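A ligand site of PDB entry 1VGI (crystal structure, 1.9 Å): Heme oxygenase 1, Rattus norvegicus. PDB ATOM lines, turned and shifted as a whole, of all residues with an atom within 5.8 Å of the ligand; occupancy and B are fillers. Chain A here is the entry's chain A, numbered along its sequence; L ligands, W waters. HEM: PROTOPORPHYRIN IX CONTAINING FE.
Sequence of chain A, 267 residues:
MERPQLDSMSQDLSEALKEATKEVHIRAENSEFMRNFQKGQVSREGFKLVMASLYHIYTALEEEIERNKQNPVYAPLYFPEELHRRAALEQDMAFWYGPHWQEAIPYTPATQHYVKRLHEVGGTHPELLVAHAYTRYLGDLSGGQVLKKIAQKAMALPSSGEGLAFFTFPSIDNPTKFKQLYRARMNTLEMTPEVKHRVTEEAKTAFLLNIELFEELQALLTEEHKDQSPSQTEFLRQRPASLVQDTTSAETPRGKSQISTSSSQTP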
ATOM      1  N   SER A  14     -19.870 -18.136 -32.638  1.00  0.00           N
ATOM      2  CA  SER A  14     -19.682 -18.646 -31.288  1.00  0.00           C
ATOM      3  C   SER A  14     -18.702 -19.817 -31.251  1.00  0.00           C
ATOM      4  O   SER A  14     -17.849 -19.903 -30.365  1.00  0.00           O
ATOM      5  CB  SER A  14     -21.025 -19.084 -30.680  1.00  0.00           C
ATOM      6  OG  SER A  14     -21.608 -20.136 -31.435  1.00  0.00           O
ATOM      7  N   LEU A  17     -15.166 -18.603 -32.115  1.00  0.00           N
ATOM      8  CA  LEU A  17     -14.536 -17.922 -30.984  1.00  0.00           C
ATOM      9  C   LEU A  17     -14.053 -18.903 -29.916  1.00  0.00           C
ATOM     10  O   LEU A  17     -12.949 -18.754 -29.384  1.00  0.00           O
ATOM     11  CB  LEU A  17     -15.491 -16.900 -30.367  1.00  0.00           C
ATOM     12  CG  LEU A  17     -15.559 -15.545 -31.096  1.00  0.00           C
ATOM     13  CD1 LEU A  17     -16.725 -14.716 -30.545  1.00  0.00           C
ATOM     14  CD2 LEU A  17     -14.246 -14.793 -30.891  1.00  0.00           C
ATOM     15  N   LYS A  18     -14.873 -19.896 -29.593  1.00  0.00           N
ATOM     16  CA  LYS A  18     -14.487 -20.880 -28.593  1.00  0.00           C
ATOM     17  C   LYS A  18     -13.229 -21.606 -29.054  1.00  0.00           C
ATOM     18  O   LYS A  18     -12.282 -21.795 -28.297  1.00  0.00           O
ATOM     19  CB  LYS A  18     -15.604 -21.900 -28.354  1.00  0.00           C
ATOM     20  CG  LYS A  18     -15.326 -22.877 -27.215  1.00  0.00           C
ATOM     21  CD  LYS A  18     -16.515 -23.799 -26.980  1.00  0.00           C
ATOM     22  CE  LYS A  18     -16.261 -24.731 -25.802  1.00  0.00           C
ATOM     23  NZ  LYS A  18     -17.419 -25.660 -25.563  1.00  0.00           N
ATOM     24  N   THR A  21     -10.042 -19.310 -29.014  1.00  0.00           N
ATOM     25  CA  THR A  21      -9.509 -18.933 -27.707  1.00  0.00           C
ATOM     26  C   THR A  21      -9.319 -20.051 -26.697  1.00  0.00           C
ATOM     27  O   THR A  21      -8.880 -19.801 -25.581  1.00  0.00           O
ATOM     28  CB  THR A  21     -10.397 -17.836 -27.053  1.00  0.00           C
ATOM     29  OG1 THR A  21     -11.696 -18.362 -26.790  1.00  0.00           O
ATOM     30  CG2 THR A  21     -10.515 -16.631 -27.975  1.00  0.00           C
ATOM     31  N   HIS A  25      -6.985 -19.531 -23.428  1.00  0.00           N
ATOM     32  CA  HIS A  25      -7.770 -19.566 -22.192  1.00  0.00           C
ATOM     33  C   HIS A  25      -7.034 -20.447 -21.183  1.00  0.00           C
ATOM     34  O   HIS A  25      -6.952 -20.125 -19.995  1.00  0.00           O
ATOM     35  CB  HIS A  25      -9.176 -20.121 -22.436  1.00  0.00           C
ATOM     36  CG  HIS A  25     -10.011 -20.178 -21.198  1.00  0.00           C
ATOM     37  ND1 HIS A  25      -9.858 -21.144 -20.225  1.00  0.00           N
ATOM     38  CD2 HIS A  25     -10.979 -19.346 -20.739  1.00  0.00           C
ATOM     39  CE1 HIS A  25     -10.693 -20.909 -19.232  1.00  0.00           C
ATOM     40  NE2 HIS A  25     -11.385 -19.829 -19.510  1.00  0.00           N
ATOM     41  N   ALA A  28      -4.367 -18.461 -19.700  1.00  0.00           N
ATOM     42  CA  ALA A  28      -4.887 -17.406 -18.844  1.00  0.00           C
ATOM     43  C   ALA A  28      -5.348 -17.951 -17.497  1.00  0.00           C
ATOM     44  O   ALA A  28      -5.005 -17.403 -16.453  1.00  0.00           O
ATOM     45  CB  ALA A  28      -6.059 -16.694 -19.538  1.00  0.00           C
ATOM     46  N   GLU A  29      -6.112 -19.039 -17.522  1.00  0.00           N
ATOM     47  CA  GLU A  29      -6.603 -19.620 -16.288  1.00  0.00           C
ATOM     48  C   GLU A  29      -5.495 -20.249 -15.456  1.00  0.00           C
ATOM     49  O   GLU A  29      -5.675 -20.525 -14.264  1.00  0.00           O
ATOM     50  CB  GLU A  29      -7.689 -20.653 -16.577  1.00  0.00           C
ATOM     51  CG  GLU A  29      -7.225 -21.918 -17.251  1.00  0.00           C
ATOM     52  CD  GLU A  29      -8.369 -22.858 -17.553  1.00  0.00           C
ATOM     53  OE1 GLU A  29      -9.134 -23.173 -16.612  1.00  0.00           O
ATOM     54  OE2 GLU A  29      -8.504 -23.283 -18.733  1.00  0.00           O
ATOM     55  N   ASN A  30      -4.343 -20.466 -16.073  1.00  0.00           N
ATOM     56  CA  ASN A  30      -3.209 -21.051 -15.361  1.00  0.00           C
ATOM     57  C   ASN A  30      -2.093 -20.050 -15.137  1.00  0.00           C
ATOM     58  O   ASN A  30      -0.967 -20.432 -14.803  1.00  0.00           O
ATOM     59  CB  ASN A  30      -2.686 -22.266 -16.123  1.00  0.00           C
ATOM     60  CG  ASN A  30      -3.592 -23.462 -15.991  1.00  0.00           C
ATOM     61  OD1 ASN A  30      -3.650 -24.100 -14.930  1.00  0.00           O
ATOM     62  ND2 ASN A  30      -4.331 -23.780 -17.042  1.00  0.00           N
ATOM     63  N   MET A  34      -3.793 -16.045 -11.252  1.00  0.00           N
ATOM     64  CA  MET A  34      -5.016 -16.827 -11.104  1.00  0.00           C
ATOM     65  C   MET A  34      -4.728 -18.091 -10.299  1.00  0.00           C
ATOM     66  O   MET A  34      -5.601 -18.595  -9.591  1.00  0.00           O
ATOM     67  CB  MET A  34      -5.596 -17.198 -12.473  1.00  0.00           C
ATOM     68  CG  MET A  34      -6.176 -16.004 -13.203  1.00  0.00           C
ATOM     69  SD  MET A  34      -7.418 -15.152 -12.197  1.00  0.00           S
ATOM     70  CE  MET A  34      -8.613 -14.662 -13.448  1.00  0.00           C
ATOM     71  N   GLN A  38      -6.693 -18.954  -6.930  1.00  0.00           N
ATOM     72  CA  GLN A  38      -7.397 -20.215  -6.753  1.00  0.00           C
ATOM     73  C   GLN A  38      -6.907 -20.966  -5.520  1.00  0.00           C
ATOM     74  O   GLN A  38      -7.567 -21.882  -5.039  1.00  0.00           O
ATOM     75  CB  GLN A  38      -7.264 -21.087  -7.996  1.00  0.00           C
ATOM     76  CG  GLN A  38      -7.831 -20.457  -9.244  1.00  0.00           C
ATOM     77  CD  GLN A  38      -7.661 -21.330 -10.468  1.00  0.00           C
ATOM     78  OE1 GLN A  38      -8.293 -22.389 -10.575  1.00  0.00           O
ATOM     79  NE2 GLN A  38      -6.809 -20.907 -11.387  1.00  0.00           N
ATOM     80  N   TYR A 114      -4.901  -1.819 -21.953  1.00  0.00           N
ATOM     81  CA  TYR A 114      -6.157  -2.512 -22.242  1.00  0.00           C
ATOM     82  C   TYR A 114      -7.222  -1.463 -22.633  1.00  0.00           C
ATOM     83  O   TYR A 114      -7.849  -1.572 -23.677  1.00  0.00           O
ATOM     84  CB  TYR A 114      -6.603  -3.280 -20.985  1.00  0.00           C
ATOM     85  CG  TYR A 114      -7.569  -4.439 -21.207  1.00  0.00           C
ATOM     86  CD1 TYR A 114      -8.552  -4.386 -22.181  1.00  0.00           C
ATOM     87  CD2 TYR A 114      -7.522  -5.556 -20.372  1.00  0.00           C
ATOM     88  CE1 TYR A 114      -9.488  -5.430 -22.321  1.00  0.00           C
ATOM     89  CE2 TYR A 114      -8.441  -6.588 -20.502  1.00  0.00           C
ATOM     90  CZ  TYR A 114      -9.427  -6.518 -21.469  1.00  0.00           C
ATOM     91  OH  TYR A 114     -10.342  -7.535 -21.580  1.00  0.00           O
ATOM     92  N   TYR A 134     -17.442 -10.473 -25.562  1.00  0.00           N
ATOM     93  CA  TYR A 134     -17.419 -11.925 -25.437  1.00  0.00           C
ATOM     94  C   TYR A 134     -16.371 -12.364 -24.405  1.00  0.00           C
ATOM     95  O   TYR A 134     -16.672 -13.096 -23.451  1.00  0.00           O
ATOM     96  CB  TYR A 134     -17.085 -12.539 -26.799  1.00  0.00           C
ATOM     97  CG  TYR A 134     -16.533 -13.944 -26.735  1.00  0.00           C
ATOM     98  CD1 TYR A 134     -17.384 -15.046 -26.615  1.00  0.00           C
ATOM     99  CD2 TYR A 134     -15.164 -14.179 -26.810  1.00  0.00           C
ATOM    100  CE1 TYR A 134     -16.879 -16.353 -26.570  1.00  0.00           C
ATOM    101  CE2 TYR A 134     -14.641 -15.475 -26.757  1.00  0.00           C
ATOM    102  CZ  TYR A 134     -15.503 -16.556 -26.640  1.00  0.00           C
ATOM    103  OH  TYR A 134     -14.987 -17.831 -26.612  1.00  0.00           O
ATOM    104  N   THR A 135     -15.151 -11.890 -24.585  1.00  0.00           N
ATOM    105  CA  THR A 135     -14.065 -12.265 -23.684  1.00  0.00           C
ATOM    106  C   THR A 135     -14.354 -11.925 -22.227  1.00  0.00           C
ATOM    107  O   THR A 135     -14.132 -12.741 -21.339  1.00  0.00           O
ATOM    108  CB  THR A 135     -12.736 -11.590 -24.129  1.00  0.00           C
ATOM    109  OG1 THR A 135     -12.377 -12.077 -25.438  1.00  0.00           O
ATOM    110  CG2 THR A 135     -11.600 -11.930 -23.157  1.00  0.00           C
ATOM    111  N   ARG A 136     -14.870 -10.720 -21.985  1.00  0.00           N
ATOM    112  CA  ARG A 136     -15.163 -10.308 -20.619  1.00  0.00           C
ATOM    113  C   ARG A 136     -16.421 -10.946 -20.019  1.00  0.00           C
ATOM    114  O   ARG A 136     -16.343 -11.685 -19.045  1.00  0.00           O
ATOM    115  CB  ARG A 136     -15.284  -8.782 -20.550  1.00  0.00           C
ATOM    116  CG  ARG A 136     -13.983  -8.043 -20.870  1.00  0.00           C
ATOM    117  CD  ARG A 136     -13.356  -7.489 -19.597  1.00  0.00           C
ATOM    118  NE  ARG A 136     -13.122  -8.518 -18.591  1.00  0.00           N
ATOM    119  CZ  ARG A 136     -11.907  -8.939 -18.224  1.00  0.00           C
ATOM    120  NH1 ARG A 136     -10.839  -8.415 -18.805  1.00  0.00           N
ATOM    121  NH2 ARG A 136     -11.772  -9.863 -17.280  1.00  0.00           N
ATOM    122  N   LEU A 138     -18.662 -13.421 -21.104  1.00  0.00           N
ATOM    123  CA  LEU A 138     -18.817 -14.879 -21.052  1.00  0.00           C
ATOM    124  C   LEU A 138     -17.893 -15.463 -20.001  1.00  0.00           C
ATOM    125  O   LEU A 138     -18.204 -16.485 -19.385  1.00  0.00           O
ATOM    126  CB  LEU A 138     -18.542 -15.530 -22.410  1.00  0.00           C
ATOM    127  CG  LEU A 138     -19.647 -15.403 -23.464  1.00  0.00           C
ATOM    128  CD1 LEU A 138     -19.888 -16.768 -24.093  1.00  0.00           C
ATOM    129  CD2 LEU A 138     -20.945 -14.888 -22.839  1.00  0.00           C
ATOM    130  N   GLY A 139     -16.754 -14.802 -19.773  1.00  0.00           N
ATOM    131  CA  GLY A 139     -15.833 -15.271 -18.759  1.00  0.00           C
ATOM    132  C   GLY A 139     -16.430 -15.047 -17.386  1.00  0.00           C
ATOM    133  O   GLY A 139     -16.367 -15.914 -16.509  1.00  0.00           O
ATOM    134  N   ASP A 140     -17.016 -13.860 -17.189  1.00  0.00           N
ATOM    135  CA  ASP A 140     -17.632 -13.522 -15.913  1.00  0.00           C
ATOM    136  C   ASP A 140     -18.705 -14.536 -15.562  1.00  0.00           C
ATOM    137  O   ASP A 140     -18.868 -14.907 -14.399  1.00  0.00           O
ATOM    138  CB  ASP A 140     -18.277 -12.130 -15.969  1.00  0.00           C
ATOM    139  CG  ASP A 140     -17.255 -11.021 -16.073  1.00  0.00           C
ATOM    140  OD1 ASP A 140     -16.167 -11.166 -15.479  1.00  0.00           O
ATOM    141  OD2 ASP A 140     -17.551 -10.015 -16.742  1.00  0.00           O
ATOM    142  N   SER A 142     -18.708 -17.557 -16.263  1.00  0.00           N
ATOM    143  CA  SER A 142     -18.117 -18.879 -16.140  1.00  0.00           C
ATOM    144  C   SER A 142     -17.125 -18.934 -14.997  1.00  0.00           C
ATOM    145  O   SER A 142     -17.502 -19.140 -13.835  1.00  0.00           O
ATOM    146  CB  SER A 142     -17.424 -19.248 -17.460  1.00  0.00           C
ATOM    147  OG  SER A 142     -18.319 -19.150 -18.552  1.00  0.00           O
ATOM    148  N   GLY A 143     -15.841 -18.754 -15.312  1.00  0.00           N
ATOM    149  CA  GLY A 143     -14.822 -18.800 -14.283  1.00  0.00           C
ATOM    150  C   GLY A 143     -15.058 -17.805 -13.172  1.00  0.00           C
ATOM    151  O   GLY A 143     -14.702 -18.050 -12.023  1.00  0.00           O
ATOM    152  N   GLY A 144     -15.648 -16.666 -13.514  1.00  0.00           N
ATOM    153  CA  GLY A 144     -15.928 -15.650 -12.526  1.00  0.00           C
ATOM    154  C   GLY A 144     -16.776 -16.167 -11.381  1.00  0.00           C
ATOM    155  O   GLY A 144     -16.612 -15.746 -10.231  1.00  0.00           O
ATOM    156  N   VAL A 146     -16.786 -19.299 -10.205  1.00  0.00           N
ATOM    157  CA  VAL A 146     -16.024 -20.181  -9.338  1.00  0.00           C
ATOM    158  C   VAL A 146     -15.091 -19.301  -8.501  1.00  0.00           C
ATOM    159  O   VAL A 146     -14.879 -19.548  -7.315  1.00  0.00           O
ATOM    160  CB  VAL A 146     -15.190 -21.223 -10.123  1.00  0.00           C
ATOM    161  CG1 VAL A 146     -16.066 -21.881 -11.193  1.00  0.00           C
ATOM    162  CG2 VAL A 146     -13.971 -20.575 -10.738  1.00  0.00           C
ATOM    163  N   LEU A 147     -14.565 -18.243  -9.123  1.00  0.00           N
ATOM    164  CA  LEU A 147     -13.663 -17.333  -8.424  1.00  0.00           C
ATOM    165  C   LEU A 147     -14.388 -16.647  -7.266  1.00  0.00           C
ATOM    166  O   LEU A 147     -13.796 -16.428  -6.212  1.00  0.00           O
ATOM    167  CB  LEU A 147     -13.127 -16.265  -9.376  1.00  0.00           C
ATOM    168  CG  LEU A 147     -12.126 -16.772 -10.428  1.00  0.00           C
ATOM    169  CD1 LEU A 147     -11.619 -15.606 -11.262  1.00  0.00           C
ATOM    170  CD2 LEU A 147     -10.975 -17.458  -9.703  1.00  0.00           C
ATOM    171  N   LYS A 179     -25.764 -17.702 -21.257  1.00  0.00           N
ATOM    172  CA  LYS A 179     -24.615 -17.854 -22.135  1.00  0.00           C
ATOM    173  C   LYS A 179     -25.046 -18.466 -23.463  1.00  0.00           C
ATOM    174  O   LYS A 179     -24.568 -18.084 -24.522  1.00  0.00           O
ATOM    175  CB  LYS A 179     -23.547 -18.744 -21.489  1.00  0.00           C
ATOM    176  CG  LYS A 179     -22.807 -18.097 -20.329  1.00  0.00           C
ATOM    177  CD  LYS A 179     -21.610 -18.958 -19.924  1.00  0.00           C
ATOM    178  CE  LYS A 179     -20.695 -19.153 -21.128  1.00  0.00           C
ATOM    179  NZ  LYS A 179     -19.527 -20.037 -20.840  1.00  0.00           N
ATOM    180  N   ARG A 183     -24.608 -16.774 -26.984  1.00  0.00           N
ATOM    181  CA  ARG A 183     -23.908 -17.415 -28.103  1.00  0.00           C
ATOM    182  C   ARG A 183     -24.787 -17.404 -29.345  1.00  0.00           C
ATOM    183  O   ARG A 183     -24.341 -17.096 -30.456  1.00  0.00           O
ATOM    184  CB  ARG A 183     -23.525 -18.859 -27.766  1.00  0.00           C
ATOM    185  CG  ARG A 183     -22.464 -19.016 -26.690  1.00  0.00           C
ATOM    186  CD  ARG A 183     -21.973 -20.464 -26.658  1.00  0.00           C
ATOM    187  NE  ARG A 183     -21.020 -20.701 -25.574  1.00  0.00           N
ATOM    188  CZ  ARG A 183     -21.355 -20.938 -24.317  1.00  0.00           C
ATOM    189  NH1 ARG A 183     -22.641 -20.990 -23.966  1.00  0.00           N
ATOM    190  NH2 ARG A 183     -20.416 -21.128 -23.405  1.00  0.00           N
ATOM    191  N   PHE A 207      -7.571 -11.721 -24.668  1.00  0.00           N
ATOM    192  CA  PHE A 207      -7.038 -12.633 -23.659  1.00  0.00           C
ATOM    193  C   PHE A 207      -5.602 -12.254 -23.300  1.00  0.00           C
ATOM    194  O   PHE A 207      -5.215 -12.320 -22.141  1.00  0.00           O
ATOM    195  CB  PHE A 207      -7.054 -14.084 -24.159  1.00  0.00           C
ATOM    196  CG  PHE A 207      -8.332 -14.826 -23.847  1.00  0.00           C
ATOM    197  CD1 PHE A 207      -9.429 -14.746 -24.708  1.00  0.00           C
ATOM    198  CD2 PHE A 207      -8.426 -15.615 -22.707  1.00  0.00           C
ATOM    199  CE1 PHE A 207     -10.600 -15.439 -24.429  1.00  0.00           C
ATOM    200  CE2 PHE A 207      -9.599 -16.313 -22.420  1.00  0.00           C
ATOM    201  CZ  PHE A 207     -10.684 -16.227 -23.288  1.00  0.00           C
ATOM    202  N   ASN A 210      -5.383  -9.433 -20.998  1.00  0.00           N
ATOM    203  CA  ASN A 210      -5.725  -9.905 -19.661  1.00  0.00           C
ATOM    204  C   ASN A 210      -4.538 -10.610 -19.028  1.00  0.00           C
ATOM    205  O   ASN A 210      -4.235 -10.405 -17.849  1.00  0.00           O
ATOM    206  CB  ASN A 210      -6.916 -10.854 -19.730  1.00  0.00           C
ATOM    207  CG  ASN A 210      -8.231 -10.122 -19.704  1.00  0.00           C
ATOM    208  OD1 ASN A 210      -8.687  -9.706 -18.639  1.00  0.00           O
ATOM    209  ND2 ASN A 210      -8.836  -9.931 -20.873  1.00  0.00           N
ATOM    210  N   PHE A 214      -2.540  -9.502 -15.566  1.00  0.00           N
ATOM    211  CA  PHE A 214      -2.271 -10.410 -14.463  1.00  0.00           C
ATOM    212  C   PHE A 214      -0.791 -10.541 -14.154  1.00  0.00           C
ATOM    213  O   PHE A 214      -0.388 -10.575 -12.987  1.00  0.00           O
ATOM    214  CB  PHE A 214      -2.829 -11.815 -14.762  1.00  0.00           C
ATOM    215  CG  PHE A 214      -4.327 -11.868 -14.802  1.00  0.00           C
ATOM    216  CD1 PHE A 214      -5.099 -11.023 -14.016  1.00  0.00           C
ATOM    217  CD2 PHE A 214      -4.978 -12.794 -15.625  1.00  0.00           C
ATOM    218  CE1 PHE A 214      -6.486 -11.096 -14.032  1.00  0.00           C
ATOM    219  CE2 PHE A 214      -6.364 -12.876 -15.644  1.00  0.00           C
ATOM    220  CZ  PHE A 214      -7.120 -12.025 -14.842  1.00  0.00           C
HETATM  221  CHA HEM L   1     -15.221 -20.289 -20.265  1.00  0.00           C
HETATM  222  CHB HEM L   1     -13.071 -21.343 -16.084  1.00  0.00           C
HETATM  223  CHC HEM L   1     -10.269 -17.418 -16.531  1.00  0.00           C
HETATM  224  CHD HEM L   1     -12.837 -16.066 -20.367  1.00  0.00           C
HETATM  225  C1A HEM L   1     -14.885 -20.943 -19.075  1.00  0.00           C
HETATM  226  C2A HEM L   1     -15.478 -22.182 -18.608  1.00  0.00           C
HETATM  227  C3A HEM L   1     -14.984 -22.397 -17.360  1.00  0.00           C
HETATM  228  C4A HEM L   1     -13.937 -21.381 -17.155  1.00  0.00           C
HETATM  229  CMA HEM L   1     -15.375 -23.430 -16.340  1.00  0.00           C
HETATM  230  CAA HEM L   1     -16.466 -23.064 -19.389  1.00  0.00           C
HETATM  231  CBA HEM L   1     -17.964 -22.606 -19.304  1.00  0.00           C
HETATM  232  CGA HEM L   1     -18.862 -23.017 -20.342  1.00  0.00           C
HETATM  233  O1A HEM L   1     -18.394 -23.802 -21.262  1.00  0.00           O
HETATM  234  O2A HEM L   1     -20.060 -22.639 -20.389  1.00  0.00           O
HETATM  235  C1B HEM L   1     -12.156 -20.317 -15.811  1.00  0.00           C
HETATM  236  C2B HEM L   1     -11.349 -20.250 -14.604  1.00  0.00           C
HETATM  237  C3B HEM L   1     -10.447 -19.247 -14.805  1.00  0.00           C
HETATM  238  C4B HEM L   1     -10.856 -18.579 -16.037  1.00  0.00           C
HETATM  239  CMB HEM L   1     -11.528 -21.160 -13.404  1.00  0.00           C
HETATM  240  CAB HEM L   1      -9.229 -18.887 -13.983  1.00  0.00           C
HETATM  241  CBB HEM L   1      -9.546 -18.000 -12.760  1.00  0.00           C
HETATM  242  C1C HEM L   1     -10.691 -16.727 -17.642  1.00  0.00           C
HETATM  243  C2C HEM L   1     -10.098 -15.487 -18.110  1.00  0.00           C
HETATM  244  C3C HEM L   1     -10.871 -15.088 -19.148  1.00  0.00           C
HETATM  245  C4C HEM L   1     -11.874 -16.101 -19.366  1.00  0.00           C
HETATM  246  CMC HEM L   1      -8.866 -14.833 -17.507  1.00  0.00           C
HETATM  247  CAC HEM L   1     -10.717 -13.818 -19.984  1.00  0.00           C
HETATM  248  CBC HEM L   1     -11.227 -12.546 -19.216  1.00  0.00           C
HETATM  249  C1D HEM L   1     -13.699 -17.115 -20.718  1.00  0.00           C
HETATM  250  C2D HEM L   1     -14.589 -17.096 -21.879  1.00  0.00           C
HETATM  251  C3D HEM L   1     -15.273 -18.259 -21.821  1.00  0.00           C
HETATM  252  C4D HEM L   1     -14.779 -19.008 -20.643  1.00  0.00           C
HETATM  253  CMD HEM L   1     -14.650 -15.971 -22.871  1.00  0.00           C
HETATM  254  CAD HEM L   1     -16.362 -18.783 -22.715  1.00  0.00           C
HETATM  255  CBD HEM L   1     -15.804 -19.678 -23.904  1.00  0.00           C
HETATM  256  CGD HEM L   1     -16.834 -20.066 -24.801  1.00  0.00           C
HETATM  257  O1D HEM L   1     -16.800 -19.663 -25.998  1.00  0.00           O
HETATM  258  O2D HEM L   1     -17.776 -20.811 -24.421  1.00  0.00           O
HETATM  259  NA  HEM L   1     -13.944 -20.469 -18.190  1.00  0.00           N
HETATM  260  NB  HEM L   1     -11.898 -19.258 -16.645  1.00  0.00           N
HETATM  261  NC  HEM L   1     -11.758 -17.132 -18.465  1.00  0.00           N
HETATM  262  ND  HEM L   1     -13.825 -18.290 -19.990  1.00  0.00           N
HETATM  263 FE   HEM L   1     -12.834 -18.793 -18.337  1.00  0.00          FE
HETATM  264  O   HOH W   1     -14.194 -17.723 -17.119  1.00  0.00           O
HETATM  265  O   HOH W   2     -18.912 -19.966 -27.526  1.00  0.00           O
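Residues that only touch the ligand: Arg 136, Leu 147, Gly 143, Gly 139, Ser 142, Lys 18, Glu 29, Met 34, Thr 135, Phe 207, Val 146, Phe 214, Asn 210, Leu 138 and Ala 28. 19 residues have an atom within 4 Å of the ligand: Lys 18, His 25, Ala 28, Glu 29, Met 34, Tyr 134, Thr 135, Arg 136, Leu 138, Gly 139, Ser 142, Gly 143, Val 146, Leu 147, Lys 179, Arg 183, Phe 207, Asn 210 and Phe 214.
A ring nitrogen (NE2) of His 25 is bound to an iron atom (FE) of the ligand (2.1 Å). The side-chain hydroxyl of Tyr 134 sits at hydrogen-bond distance from an oxygen (O1D) of the ligand, at 2.6 Å. The side-chain amino group (NZ) of Lys 179 is in salt-bridge range of an oxygen (O2A) of the ligand (2.7 Å). NH2 of Arg 183 lies within salt-bridge range of O2D of the ligand (2.8 Å).
A ring nitrogen (ND1) of His 25 is in hydrogen-bond range of the side-chain carboxylate of Glu 29 (2.9 Å). NZ of Lys 179 sits at hydrogen-bond distance from OG of Ser 142 (2.7 Å). NH1 of Arg 136 sits at hydrogen-bond distance from OD1 of Asn 210 (2.5 Å). The guanidinium group of Arg 136 is in hydrogen-bond range of the side-chain hydroxyl of Tyr 114 (3.0 Å). O of Gly 139 lies within hydrogen-bond range of N of Gly 144 (3.2 Å). The side-chain hydroxyl of Ser 142 is in hydrogen-bond range of the backbone carbonyl oxygen of Leu 138. O of Glu 29 lies within hydrogen-bond range of NE2 of Gln 38, at 3.1 Å. ND2 of Asn 210 is in hydrogen-bond range of OH of Tyr 114 (2.9 Å).
Water W2 lies within hydrogen-bond range of O1D of the ligand (2.6 Å), NE of Arg 183 (3.0 Å) and O of Ser 14 (3.0 Å).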
